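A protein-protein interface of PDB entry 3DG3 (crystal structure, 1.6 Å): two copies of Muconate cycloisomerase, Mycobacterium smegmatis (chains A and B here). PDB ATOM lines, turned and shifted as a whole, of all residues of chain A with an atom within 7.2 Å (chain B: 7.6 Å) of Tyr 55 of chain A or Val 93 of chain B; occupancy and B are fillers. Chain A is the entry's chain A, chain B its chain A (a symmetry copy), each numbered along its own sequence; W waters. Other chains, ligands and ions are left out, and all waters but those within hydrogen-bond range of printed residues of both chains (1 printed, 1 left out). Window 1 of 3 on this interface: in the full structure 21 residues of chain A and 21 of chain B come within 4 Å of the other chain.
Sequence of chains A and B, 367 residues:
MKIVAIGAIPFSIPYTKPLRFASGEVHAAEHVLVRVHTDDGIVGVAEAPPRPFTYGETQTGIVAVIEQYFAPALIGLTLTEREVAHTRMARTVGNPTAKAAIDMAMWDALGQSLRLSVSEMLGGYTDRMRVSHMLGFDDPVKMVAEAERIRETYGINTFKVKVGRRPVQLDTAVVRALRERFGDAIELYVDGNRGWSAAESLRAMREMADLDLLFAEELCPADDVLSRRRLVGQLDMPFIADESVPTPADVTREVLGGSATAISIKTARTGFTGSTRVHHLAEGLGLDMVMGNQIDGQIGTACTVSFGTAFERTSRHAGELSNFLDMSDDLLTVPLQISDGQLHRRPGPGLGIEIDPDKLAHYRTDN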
ATOM      1  N   PRO A  49     -16.133 -15.576  30.711  1.00  0.00           N
ATOM      2  CA  PRO A  49     -15.256 -15.310  29.571  1.00  0.00           C
ATOM      3  C   PRO A  49     -15.692 -16.099  28.338  1.00  0.00           C
ATOM      4  O   PRO A  49     -15.633 -17.325  28.331  1.00  0.00           O
ATOM      5  CB  PRO A  49     -13.894 -15.755  30.084  1.00  0.00           C
ATOM      6  CG  PRO A  49     -14.249 -16.952  30.920  1.00  0.00           C
ATOM      7  CD  PRO A  49     -15.494 -16.500  31.668  1.00  0.00           C
ATOM      8  N   PRO A  50     -16.152 -15.405  27.286  1.00  0.00           N
ATOM      9  CA  PRO A  50     -16.576 -16.129  26.083  1.00  0.00           C
ATOM     10  C   PRO A  50     -15.374 -16.693  25.334  1.00  0.00           C
ATOM     11  O   PRO A  50     -14.472 -15.955  24.934  1.00  0.00           O
ATOM     12  CB  PRO A  50     -17.324 -15.066  25.285  1.00  0.00           C
ATOM     13  CG  PRO A  50     -16.598 -13.812  25.643  1.00  0.00           C
ATOM     14  CD  PRO A  50     -16.367 -13.955  27.136  1.00  0.00           C
ATOM     15  N   ARG A  51     -15.363 -18.009  25.162  1.00  0.00           N
ATOM     16  CA  ARG A  51     -14.276 -18.684  24.471  1.00  0.00           C
ATOM     17  C   ARG A  51     -14.883 -19.537  23.362  1.00  0.00           C
ATOM     18  O   ARG A  51     -15.090 -20.737  23.524  1.00  0.00           O
ATOM     19  CB  ARG A  51     -13.498 -19.563  25.460  1.00  0.00           C
ATOM     20  CG  ARG A  51     -12.908 -18.793  26.646  1.00  0.00           C
ATOM     21  CD  ARG A  51     -11.796 -17.853  26.197  1.00  0.00           C
ATOM     22  NE  ARG A  51     -11.266 -17.017  27.279  1.00  0.00           N
ATOM     23  CZ  ARG A  51     -11.562 -15.731  27.449  1.00  0.00           C
ATOM     24  NH1 ARG A  51     -12.392 -15.116  26.615  1.00  0.00           N
ATOM     25  NH2 ARG A  51     -11.005 -15.044  28.441  1.00  0.00           N
ATOM     26  N   PRO A  52     -15.191 -18.918  22.215  1.00  0.00           N
ATOM     27  CA  PRO A  52     -15.783 -19.679  21.113  1.00  0.00           C
ATOM     28  C   PRO A  52     -14.952 -20.866  20.631  1.00  0.00           C
ATOM     29  O   PRO A  52     -15.501 -21.850  20.136  1.00  0.00           O
ATOM     30  CB  PRO A  52     -15.994 -18.618  20.027  1.00  0.00           C
ATOM     31  CG  PRO A  52     -14.979 -17.566  20.350  1.00  0.00           C
ATOM     32  CD  PRO A  52     -15.033 -17.498  21.854  1.00  0.00           C
ATOM     33  N   PHE A  53     -13.637 -20.785  20.806  1.00  0.00           N
ATOM     34  CA  PHE A  53     -12.748 -21.849  20.360  1.00  0.00           C
ATOM     35  C   PHE A  53     -12.504 -22.924  21.415  1.00  0.00           C
ATOM     36  O   PHE A  53     -11.690 -23.825  21.215  1.00  0.00           O
ATOM     37  CB  PHE A  53     -11.428 -21.231  19.893  1.00  0.00           C
ATOM     38  CG  PHE A  53     -11.612 -20.143  18.870  1.00  0.00           C
ATOM     39  CD1 PHE A  53     -10.813 -19.003  18.893  1.00  0.00           C
ATOM     40  CD2 PHE A  53     -12.612 -20.241  17.903  1.00  0.00           C
ATOM     41  CE1 PHE A  53     -11.010 -17.974  17.969  1.00  0.00           C
ATOM     42  CE2 PHE A  53     -12.816 -19.221  16.976  1.00  0.00           C
ATOM     43  CZ  PHE A  53     -12.015 -18.083  17.010  1.00  0.00           C
ATOM     44  N   THR A  54     -13.217 -22.831  22.534  1.00  0.00           N
ATOM     45  CA  THR A  54     -13.086 -23.815  23.602  1.00  0.00           C
ATOM     46  C   THR A  54     -14.452 -24.375  23.983  1.00  0.00           C
ATOM     47  O   THR A  54     -14.610 -25.590  24.144  1.00  0.00           O
ATOM     48  CB  THR A  54     -12.428 -23.205  24.861  1.00  0.00           C
ATOM     49  OG1 THR A  54     -11.097 -22.784  24.544  1.00  0.00           O
ATOM     50  CG2 THR A  54     -12.367 -24.233  25.989  1.00  0.00           C
ATOM     51  N   TYR A  55     -15.439 -23.489  24.114  1.00  0.00           N
ATOM     52  CA  TYR A  55     -16.792 -23.897  24.486  1.00  0.00           C
ATOM     53  C   TYR A  55     -17.841 -23.508  23.451  1.00  0.00           C
ATOM     54  O   TYR A  55     -18.958 -24.016  23.485  1.00  0.00           O
ATOM     55  CB  TYR A  55     -17.183 -23.285  25.830  1.00  0.00           C
ATOM     56  CG  TYR A  55     -16.209 -23.583  26.942  1.00  0.00           C
ATOM     57  CD1 TYR A  55     -15.913 -24.894  27.303  1.00  0.00           C
ATOM     58  CD2 TYR A  55     -15.575 -22.549  27.627  1.00  0.00           C
ATOM     59  CE1 TYR A  55     -15.003 -25.170  28.322  1.00  0.00           C
ATOM     60  CE2 TYR A  55     -14.664 -22.813  28.646  1.00  0.00           C
ATOM     61  CZ  TYR A  55     -14.384 -24.124  28.986  1.00  0.00           C
ATOM     62  OH  TYR A  55     -13.477 -24.385  29.987  1.00  0.00           O
ATOM     63  N   GLY A  56     -17.490 -22.594  22.551  1.00  0.00           N
ATOM     64  CA  GLY A  56     -18.436 -22.171  21.533  1.00  0.00           C
ATOM     65  C   GLY A  56     -19.327 -21.012  21.939  1.00  0.00           C
ATOM     66  O   GLY A  56     -20.239 -20.638  21.204  1.00  0.00           O
ATOM     67  N   GLU A  57     -19.072 -20.438  23.110  1.00  0.00           N
ATOM     68  CA  GLU A  57     -19.864 -19.308  23.582  1.00  0.00           C
ATOM     69  C   GLU A  57     -19.311 -18.001  23.022  1.00  0.00           C
ATOM     70  O   GLU A  57     -18.113 -17.888  22.752  1.00  0.00           O
ATOM     71  CB  GLU A  57     -19.837 -19.235  25.115  1.00  0.00           C
ATOM     72  CG  GLU A  57     -20.530 -20.380  25.831  1.00  0.00           C
ATOM     73  CD  GLU A  57     -20.437 -20.254  27.342  1.00  0.00           C
ATOM     74  OE1 GLU A  57     -19.338 -20.471  27.895  1.00  0.00           O
ATOM     75  OE2 GLU A  57     -21.461 -19.933  27.978  1.00  0.00           O
ATOM     76  N   THR A  58     -20.191 -17.023  22.832  1.00  0.00           N
ATOM     77  CA  THR A  58     -19.783 -15.709  22.346  1.00  0.00           C
ATOM     78  C   THR A  58     -20.256 -14.713  23.392  1.00  0.00           C
ATOM     79  O   THR A  58     -21.122 -15.028  24.209  1.00  0.00           O
ATOM     80  CB  THR A  58     -20.445 -15.345  20.995  1.00  0.00           C
ATOM     81  OG1 THR A  58     -21.862 -15.218  21.170  1.00  0.00           O
ATOM     82  CG2 THR A  58     -20.148 -16.413  19.953  1.00  0.00           C
ATOM     83  N   GLY A  94     -24.672 -27.160  27.410  1.00  0.00           N
ATOM     84  CA  GLY A  94     -23.564 -26.254  27.162  1.00  0.00           C
ATOM     85  C   GLY A  94     -23.633 -24.944  27.924  1.00  0.00           C
ATOM     86  O   GLY A  94     -24.056 -24.921  29.080  1.00  0.00           O
ATOM     87  N   ASN A  95     -23.220 -23.858  27.268  1.00  0.00           N
ATOM     88  CA  ASN A  95     -23.216 -22.524  27.876  1.00  0.00           C
ATOM     89  C   ASN A  95     -22.542 -22.607  29.240  1.00  0.00           C
ATOM     90  O   ASN A  95     -23.046 -22.068  30.228  1.00  0.00           O
ATOM     91  CB  ASN A  95     -24.652 -22.018  28.042  1.00  0.00           C
ATOM     92  CG  ASN A  95     -25.351 -21.811  26.716  1.00  0.00           C
ATOM     93  OD1 ASN A  95     -25.239 -20.751  26.099  1.00  0.00           O
ATOM     94  ND2 ASN A  95     -26.066 -22.836  26.258  1.00  0.00           N
ATOM     95  N   PRO A  96     -21.372 -23.261  29.302  1.00  0.00           N
ATOM     96  CA  PRO A  96     -20.650 -23.417  30.565  1.00  0.00           C
ATOM     97  C   PRO A  96     -20.289 -22.175  31.374  1.00  0.00           C
ATOM     98  O   PRO A  96     -20.577 -22.130  32.568  1.00  0.00           O
ATOM     99  CB  PRO A  96     -19.422 -24.233  30.162  1.00  0.00           C
ATOM    100  CG  PRO A  96     -19.169 -23.789  28.765  1.00  0.00           C
ATOM    101  CD  PRO A  96     -20.560 -23.760  28.176  1.00  0.00           C
ATOM    102  N   THR A  97     -19.672 -21.172  30.755  1.00  0.00           N
ATOM    103  CA  THR A  97     -19.284 -20.002  31.536  1.00  0.00           C
ATOM    104  C   THR A  97     -20.477 -19.181  31.994  1.00  0.00           C
ATOM    105  O   THR A  97     -20.419 -18.537  33.040  1.00  0.00           O
ATOM    106  CB  THR A  97     -18.265 -19.093  30.791  1.00  0.00           C
ATOM    107  OG1 THR A  97     -18.891 -18.443  29.678  1.00  0.00           O
ATOM    108  CG2 THR A  97     -17.080 -19.921  30.305  1.00  0.00           C
ATOM    109  N   ARG A 194      -4.176 -28.892  22.205  1.00  0.00           N
ATOM    110  CA  ARG A 194      -4.548 -29.743  21.069  1.00  0.00           C
ATOM    111  C   ARG A 194      -3.797 -29.440  19.774  1.00  0.00           C
ATOM    112  O   ARG A 194      -4.201 -29.892  18.700  1.00  0.00           O
ATOM    113  CB  ARG A 194      -6.049 -29.622  20.793  1.00  0.00           C
ATOM    114  CG  ARG A 194      -6.928 -29.689  22.028  1.00  0.00           C
ATOM    115  CD  ARG A 194      -8.399 -29.723  21.644  1.00  0.00           C
ATOM    116  NE  ARG A 194      -8.776 -28.621  20.762  1.00  0.00           N
ATOM    117  CZ  ARG A 194      -8.740 -27.340  21.112  1.00  0.00           C
ATOM    118  NH1 ARG A 194      -8.342 -26.993  22.326  1.00  0.00           N
ATOM    119  NH2 ARG A 194      -9.104 -26.403  20.245  1.00  0.00           N
ATOM    120  N   ASP A 242      -8.321 -30.959  29.812  1.00  0.00           N
ATOM    121  CA  ASP A 242      -8.837 -29.635  30.134  1.00  0.00           C
ATOM    122  C   ASP A 242     -10.079 -29.344  29.296  1.00  0.00           C
ATOM    123  O   ASP A 242     -11.202 -29.589  29.740  1.00  0.00           O
ATOM    124  CB  ASP A 242      -7.722 -28.613  29.856  1.00  0.00           C
ATOM    125  CG  ASP A 242      -8.154 -27.169  30.056  1.00  0.00           C
ATOM    126  OD1 ASP A 242      -9.323 -26.906  30.393  1.00  0.00           O
ATOM    127  OD2 ASP A 242      -7.298 -26.283  29.858  1.00  0.00           O
ATOM    128  N   GLU A 243      -9.887 -28.853  28.076  1.00  0.00           N
ATOM    129  CA  GLU A 243     -11.035 -28.540  27.235  1.00  0.00           C
ATOM    130  C   GLU A 243     -11.881 -29.766  26.910  1.00  0.00           C
ATOM    131  O   GLU A 243     -13.054 -29.634  26.550  1.00  0.00           O
ATOM    132  CB  GLU A 243     -10.598 -27.846  25.938  1.00  0.00           C
ATOM    133  CG  GLU A 243      -9.495 -28.530  25.152  1.00  0.00           C
ATOM    134  CD  GLU A 243      -8.108 -27.992  25.479  1.00  0.00           C
ATOM    135  OE1 GLU A 243      -7.271 -27.922  24.554  1.00  0.00           O
ATOM    136  OE2 GLU A 243      -7.849 -27.648  26.650  1.00  0.00           O
ATOM    137  N   SER A 244     -11.303 -30.955  27.057  1.00  0.00           N
ATOM    138  CA  SER A 244     -12.043 -32.182  26.763  1.00  0.00           C
ATOM    139  C   SER A 244     -12.854 -32.732  27.940  1.00  0.00           C
ATOM    140  O   SER A 244     -13.565 -33.727  27.789  1.00  0.00           O
ATOM    141  CB  SER A 244     -11.093 -33.269  26.253  1.00  0.00           C
ATOM    142  OG  SER A 244     -10.107 -33.575  27.223  1.00  0.00           O
ATOM    143  N   VAL A 245     -12.756 -32.097  29.107  1.00  0.00           N
ATOM    144  CA  VAL A 245     -13.509 -32.556  30.275  1.00  0.00           C
ATOM    145  C   VAL A 245     -14.259 -31.407  30.947  1.00  0.00           C
ATOM    146  O   VAL A 245     -14.069 -31.126  32.129  1.00  0.00           O
ATOM    147  CB  VAL A 245     -12.588 -33.269  31.324  1.00  0.00           C
ATOM    148  CG1 VAL A 245     -12.140 -34.632  30.780  1.00  0.00           C
ATOM    149  CG2 VAL A 245     -11.359 -32.408  31.647  1.00  0.00           C
ATOM    150  N   PRO A 246     -15.144 -30.738  30.196  1.00  0.00           N
ATOM    151  CA  PRO A 246     -15.915 -29.613  30.736  1.00  0.00           C
ATOM    152  C   PRO A 246     -17.017 -29.999  31.728  1.00  0.00           C
ATOM    153  O   PRO A 246     -17.525 -29.143  32.454  1.00  0.00           O
ATOM    154  CB  PRO A 246     -16.468 -28.952  29.479  1.00  0.00           C
ATOM    155  CG  PRO A 246     -16.718 -30.141  28.585  1.00  0.00           C
ATOM    156  CD  PRO A 246     -15.438 -30.932  28.763  1.00  0.00           C
ATOM    157  N   LYS A 266     -11.509 -25.778  36.154  1.00  0.00           N
ATOM    158  CA  LYS A 266     -11.546 -24.345  35.888  1.00  0.00           C
ATOM    159  C   LYS A 266     -12.889 -23.829  36.359  1.00  0.00           C
ATOM    160  O   LYS A 266     -13.933 -24.235  35.850  1.00  0.00           O
ATOM    161  CB  LYS A 266     -11.359 -24.049  34.395  1.00  0.00           C
ATOM    162  CG  LYS A 266      -9.947 -24.311  33.890  1.00  0.00           C
ATOM    163  CD  LYS A 266      -9.725 -23.769  32.481  1.00  0.00           C
ATOM    164  CE  LYS A 266      -8.336 -24.147  31.964  1.00  0.00           C
ATOM    165  NZ  LYS A 266      -8.041 -23.588  30.608  1.00  0.00           N
ATOM    166  N   ALA A 268     -14.157 -21.146  35.781  1.00  0.00           N
ATOM    167  CA  ALA A 268     -14.825 -20.403  34.717  1.00  0.00           C
ATOM    168  C   ALA A 268     -15.883 -21.262  34.027  1.00  0.00           C
ATOM    169  O   ALA A 268     -16.912 -20.747  33.597  1.00  0.00           O
ATOM    170  CB  ALA A 268     -13.810 -19.904  33.689  1.00  0.00           C
ATOM    171  N   ARG A 269     -15.638 -22.565  33.925  1.00  0.00           N
ATOM    172  CA  ARG A 269     -16.601 -23.447  33.266  1.00  0.00           C
ATOM    173  C   ARG A 269     -17.450 -24.318  34.192  1.00  0.00           C
ATOM    174  O   ARG A 269     -18.517 -24.787  33.785  1.00  0.00           O
ATOM    175  CB  ARG A 269     -15.901 -24.343  32.235  1.00  0.00           C
ATOM    176  CG  ARG A 269     -14.726 -25.130  32.788  1.00  0.00           C
ATOM    177  CD  ARG A 269     -14.602 -26.508  32.140  1.00  0.00           C
ATOM    178  NE  ARG A 269     -13.438 -27.207  32.681  1.00  0.00           N
ATOM    179  CZ  ARG A 269     -12.230 -27.187  32.126  1.00  0.00           C
ATOM    180  NH1 ARG A 269     -12.023 -26.515  30.998  1.00  0.00           N
ATOM    181  NH2 ARG A 269     -11.221 -27.809  32.722  1.00  0.00           N
ATOM    182  N   THR A 270     -17.001 -24.558  35.423  1.00  0.00           N
ATOM    183  CA  THR A 270     -17.804 -25.371  36.327  1.00  0.00           C
ATOM    184  C   THR A 270     -18.168 -24.669  37.636  1.00  0.00           C
ATOM    185  O   THR A 270     -18.735 -25.285  38.530  1.00  0.00           O
ATOM    186  CB  THR A 270     -17.150 -26.765  36.616  1.00  0.00           C
ATOM    187  OG1 THR A 270     -15.768 -26.615  36.959  1.00  0.00           O
ATOM    188  CG2 THR A 270     -17.262 -27.665  35.383  1.00  0.00           C
ATOM    189  N   GLN A 294      -8.710 -19.688  32.506  1.00  0.00           N
ATOM    190  CA  GLN A 294      -9.455 -19.540  31.259  1.00  0.00           C
ATOM    191  C   GLN A 294      -9.119 -18.174  30.662  1.00  0.00           C
ATOM    192  O   GLN A 294      -9.952 -17.563  29.989  1.00  0.00           O
ATOM    193  CB  GLN A 294     -10.956 -19.607  31.553  1.00  0.00           C
ATOM    194  CG  GLN A 294     -11.806 -20.027  30.370  1.00  0.00           C
ATOM    195  CD  GLN A 294     -11.812 -21.530  30.185  1.00  0.00           C
ATOM    196  OE1 GLN A 294     -12.443 -22.256  30.954  1.00  0.00           O
ATOM    197  NE2 GLN A 294     -11.098 -22.005  29.171  1.00  0.00           N
ATOM    198  N   TYR B  55     -28.604 -28.695  22.303  1.00  0.00           N
ATOM    199  CA  TYR B  55     -27.268 -28.243  21.924  1.00  0.00           C
ATOM    200  C   TYR B  55     -26.830 -26.983  22.660  1.00  0.00           C
ATOM    201  O   TYR B  55     -25.650 -26.645  22.657  1.00  0.00           O
ATOM    202  CB  TYR B  55     -27.203 -27.975  20.421  1.00  0.00           C
ATOM    203  CG  TYR B  55     -27.632 -29.147  19.573  1.00  0.00           C
ATOM    204  CD1 TYR B  55     -26.987 -30.376  19.672  1.00  0.00           C
ATOM    205  CD2 TYR B  55     -28.694 -29.027  18.680  1.00  0.00           C
ATOM    206  CE1 TYR B  55     -27.392 -31.463  18.899  1.00  0.00           C
ATOM    207  CE2 TYR B  55     -29.107 -30.106  17.904  1.00  0.00           C
ATOM    208  CZ  TYR B  55     -28.452 -31.319  18.020  1.00  0.00           C
ATOM    209  OH  TYR B  55     -28.867 -32.387  17.259  1.00  0.00           O
ATOM    210  N   VAL B  65     -23.229 -15.919  16.189  1.00  0.00           N
ATOM    211  CA  VAL B  65     -22.041 -16.663  15.796  1.00  0.00           C
ATOM    212  C   VAL B  65     -21.837 -16.649  14.282  1.00  0.00           C
ATOM    213  O   VAL B  65     -20.705 -16.631  13.804  1.00  0.00           O
ATOM    214  CB  VAL B  65     -22.083 -18.124  16.328  1.00  0.00           C
ATOM    215  CG1 VAL B  65     -23.044 -18.971  15.502  1.00  0.00           C
ATOM    216  CG2 VAL B  65     -20.679 -18.714  16.320  1.00  0.00           C
ATOM    217  N   PHE B  70     -18.537 -17.055  11.696  1.00  0.00           N
ATOM    218  CA  PHE B  70     -18.544 -17.856  10.478  1.00  0.00           C
ATOM    219  C   PHE B  70     -18.574 -17.089   9.160  1.00  0.00           C
ATOM    220  O   PHE B  70     -17.785 -17.379   8.262  1.00  0.00           O
ATOM    221  CB  PHE B  70     -19.692 -18.871  10.527  1.00  0.00           C
ATOM    222  CG  PHE B  70     -19.600 -19.832  11.683  1.00  0.00           C
ATOM    223  CD1 PHE B  70     -18.370 -20.360  12.070  1.00  0.00           C
ATOM    224  CD2 PHE B  70     -20.743 -20.220  12.375  1.00  0.00           C
ATOM    225  CE1 PHE B  70     -18.282 -21.262  13.132  1.00  0.00           C
ATOM    226  CE2 PHE B  70     -20.667 -21.120  13.437  1.00  0.00           C
ATOM    227  CZ  PHE B  70     -19.434 -21.642  13.817  1.00  0.00           C
ATOM    228  N   MET B  89     -14.686 -23.648  10.201  1.00  0.00           N
ATOM    229  CA  MET B  89     -15.801 -23.633  11.142  1.00  0.00           C
ATOM    230  C   MET B  89     -15.495 -24.505  12.357  1.00  0.00           C
ATOM    231  O   MET B  89     -15.924 -24.204  13.468  1.00  0.00           O
ATOM    232  CB  MET B  89     -17.096 -24.120  10.473  1.00  0.00           C
ATOM    233  CG  MET B  89     -17.694 -23.134   9.476  1.00  0.00           C
ATOM    234  SD  MET B  89     -19.387 -23.548   8.991  1.00  0.00           S
ATOM    235  CE  MET B  89     -20.300 -22.624  10.166  1.00  0.00           C
ATOM    236  N   ALA B  90     -14.736 -25.576  12.137  1.00  0.00           N
ATOM    237  CA  ALA B  90     -14.388 -26.503  13.211  1.00  0.00           C
ATOM    238  C   ALA B  90     -13.553 -25.861  14.311  1.00  0.00           C
ATOM    239  O   ALA B  90     -13.420 -26.424  15.401  1.00  0.00           O
ATOM    240  CB  ALA B  90     -13.655 -27.713  12.641  1.00  0.00           C
ATOM    241  N   ARG B  91     -12.979 -24.695  14.031  1.00  0.00           N
ATOM    242  CA  ARG B  91     -12.180 -24.001  15.035  1.00  0.00           C
ATOM    243  C   ARG B  91     -13.091 -23.572  16.175  1.00  0.00           C
ATOM    244  O   ARG B  91     -12.672 -23.512  17.329  1.00  0.00           O
ATOM    245  CB  ARG B  91     -11.488 -22.774  14.438  1.00  0.00           C
ATOM    246  CG  ARG B  91     -10.430 -23.108  13.401  1.00  0.00           C
ATOM    247  CD  ARG B  91      -9.578 -21.893  13.098  1.00  0.00           C
ATOM    248  NE  ARG B  91      -8.838 -21.454  14.279  1.00  0.00           N
ATOM    249  CZ  ARG B  91      -8.061 -20.377  14.320  1.00  0.00           C
ATOM    250  NH1 ARG B  91      -7.425 -20.056  15.441  1.00  0.00           N
ATOM    251  NH2 ARG B  91      -7.922 -19.613  13.244  1.00  0.00           N
ATOM    252  N   THR B  92     -14.339 -23.262  15.840  1.00  0.00           N
ATOM    253  CA  THR B  92     -15.317 -22.868  16.842  1.00  0.00           C
ATOM    254  C   THR B  92     -15.972 -24.146  17.355  1.00  0.00           C
ATOM    255  O   THR B  92     -16.400 -24.991  16.571  1.00  0.00           O
ATOM    256  CB  THR B  92     -16.397 -21.941  16.244  1.00  0.00           C
ATOM    257  OG1 THR B  92     -15.783 -20.730  15.789  1.00  0.00           O
ATOM    258  CG2 THR B  92     -17.450 -21.596  17.288  1.00  0.00           C
ATOM    259  N   VAL B  93     -16.024 -24.292  18.674  1.00  0.00           N
ATOM    260  CA  VAL B  93     -16.619 -25.466  19.294  1.00  0.00           C
ATOM    261  C   VAL B  93     -18.139 -25.339  19.368  1.00  0.00           C
ATOM    262  O   VAL B  93     -18.669 -24.238  19.497  1.00  0.00           O
ATOM    263  CB  VAL B  93     -16.051 -25.669  20.719  1.00  0.00           C
ATOM    264  CG1 VAL B  93     -16.801 -26.777  21.438  1.00  0.00           C
ATOM    265  CG2 VAL B  93     -14.569 -26.009  20.634  1.00  0.00           C
ATOM    266  N   GLY B  94     -18.836 -26.468  19.268  1.00  0.00           N
ATOM    267  CA  GLY B  94     -20.287 -26.450  19.349  1.00  0.00           C
ATOM    268  C   GLY B  94     -20.977 -25.713  18.218  1.00  0.00           C
ATOM    269  O   GLY B  94     -20.535 -25.786  17.070  1.00  0.00           O
ATOM    270  N   ASN B  95     -22.055 -25.001  18.549  1.00  0.00           N
ATOM    271  CA  ASN B  95     -22.835 -24.245  17.563  1.00  0.00           C
ATOM    272  C   ASN B  95     -23.141 -25.152  16.379  1.00  0.00           C
ATOM    273  O   ASN B  95     -22.984 -24.756  15.222  1.00  0.00           O
ATOM    274  CB  ASN B  95     -22.038 -23.028  17.086  1.00  0.00           C
ATOM    275  CG  ASN B  95     -21.785 -22.029  18.194  1.00  0.00           C
ATOM    276  OD1 ASN B  95     -22.613 -21.157  18.462  1.00  0.00           O
ATOM    277  ND2 ASN B  95     -20.641 -22.161  18.861  1.00  0.00           N
ATOM    278  N   PRO B  96     -23.615 -26.377  16.655  1.00  0.00           N
ATOM    279  CA  PRO B  96     -23.924 -27.335  15.593  1.00  0.00           C
ATOM    280  C   PRO B  96     -24.895 -26.932  14.488  1.00  0.00           C
ATOM    281  O   PRO B  96     -24.566 -27.086  13.313  1.00  0.00           O
ATOM    282  CB  PRO B  96     -24.393 -28.567  16.367  1.00  0.00           C
ATOM    283  CG  PRO B  96     -25.028 -27.981  17.577  1.00  0.00           C
ATOM    284  CD  PRO B  96     -24.049 -26.897  17.966  1.00  0.00           C
ATOM    285  N   LYS B  99     -23.441 -24.170  12.131  1.00  0.00           N
ATOM    286  CA  LYS B  99     -22.475 -24.714  11.182  1.00  0.00           C
ATOM    287  C   LYS B  99     -23.165 -25.557  10.116  1.00  0.00           C
ATOM    288  O   LYS B  99     -22.860 -25.446   8.929  1.00  0.00           O
ATOM    289  CB  LYS B  99     -21.456 -25.608  11.891  1.00  0.00           C
ATOM    290  CG  LYS B  99     -20.522 -24.919  12.863  1.00  0.00           C
ATOM    291  CD  LYS B  99     -19.747 -25.984  13.628  1.00  0.00           C
ATOM    292  CE  LYS B  99     -18.759 -25.400  14.612  1.00  0.00           C
ATOM    293  NZ  LYS B  99     -18.150 -26.488  15.428  1.00  0.00           N
HETATM  294  O   HOH W   1     -22.828 -19.707  20.635  1.00  0.00           O
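The backbone carbonyl oxygen (O) of Gly 56 of chain A is in hydrogen-bond range of the side-chain amide nitrogen (ND2) of Asn 95 of chain B (2.8 Å). The backbone NH of Val 93 of chain B lies within hydrogen-bond range of the backbone carbonyl oxygen of Pro 52 of chain A (2.9 Å).
The side-chain amide nitrogen (ND2) of Asn 95 of chain B lies within hydrogen-bond range of the backbone carbonyl oxygen (O) of Val 93 of chain B (2.9 Å). O of Arg 51 of chain A lies within hydrogen-bond range of N of Gly 56 of chain A (3.2 Å). OE1 of Gln 294 of chain A lies within hydrogen-bond range of OH of Tyr 55 of chain A (2.6 Å). NH1 of Arg 269 of chain A lies within hydrogen-bond range of OH of Tyr 55 of chain A, 2.8 Å away. The side-chain amino group of Lys 99 of chain B lies within hydrogen-bond range of the backbone carbonyl oxygen of Thr 92 of chain B, 2.6 Å away.
Among the printed residues, merely in contact across the chains: Gly 56 of chain A with Val 93 of chain B, Phe 53 of chain A with Arg 91 of chain B, Pro 52 of chain A with Thr 92 of chain B, Phe 53 of chain A with Thr 92 of chain B, Thr 54 of chain A with Val 93 of chain B, Phe 53 of chain A with Val 93 of chain B and Tyr 55 of chain A with Val 93 of chain B.
Of chain B, only Val 93 comes within 4 Å of Tyr 55 of chain A. Val 93 of chain B touches just these residues of chain A: Pro 52 (2.9 Å), Phe 53 (3.7 Å), Thr 54 (3.5 Å), Tyr 55 (3.9 Å) and Gly 56 (2.9 Å). Of the printed residues of chain A, Arg 91 of chain B touches Phe 53. Printed residues of chain B within 4 Å of Pro 52 of chain A: Thr 92 and Val 93. Of the printed residues of chain A, Thr 92 of chain B touches Pro 52 (3.5 Å) and Phe 53 (3.5 Å). Ala 90 of chain B touches none of the printed residues of chain A. Glu 57 of chain A touches none of the printed residues of chain B. The nearest printed residue of chain B that does not touch Thr 54 of chain A is Arg 91 of chain B (5.3 Å).
Hydrophobic or aromatic side chains of chain B that line the printed part of chain A: Val 93. Hydrophobic or aromatic side chains of chain A that line the printed part of chain B: Phe 53. Among the printed residues, no Asp or Glu carboxylate lies within 4 Å of a Lys or Arg side-chain nitrogen of the other chain.
Positions printed for both chains: 55, 94, 95 and 96. Of the 9 pairs that touch across the chains among the printed residues, none has its exchanged pair printed and touching as well.
Water W1 bridges OD1 of Asn 95 of chain B (2.6 Å) and O of Gly 56 of chain A (2.8 Å).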
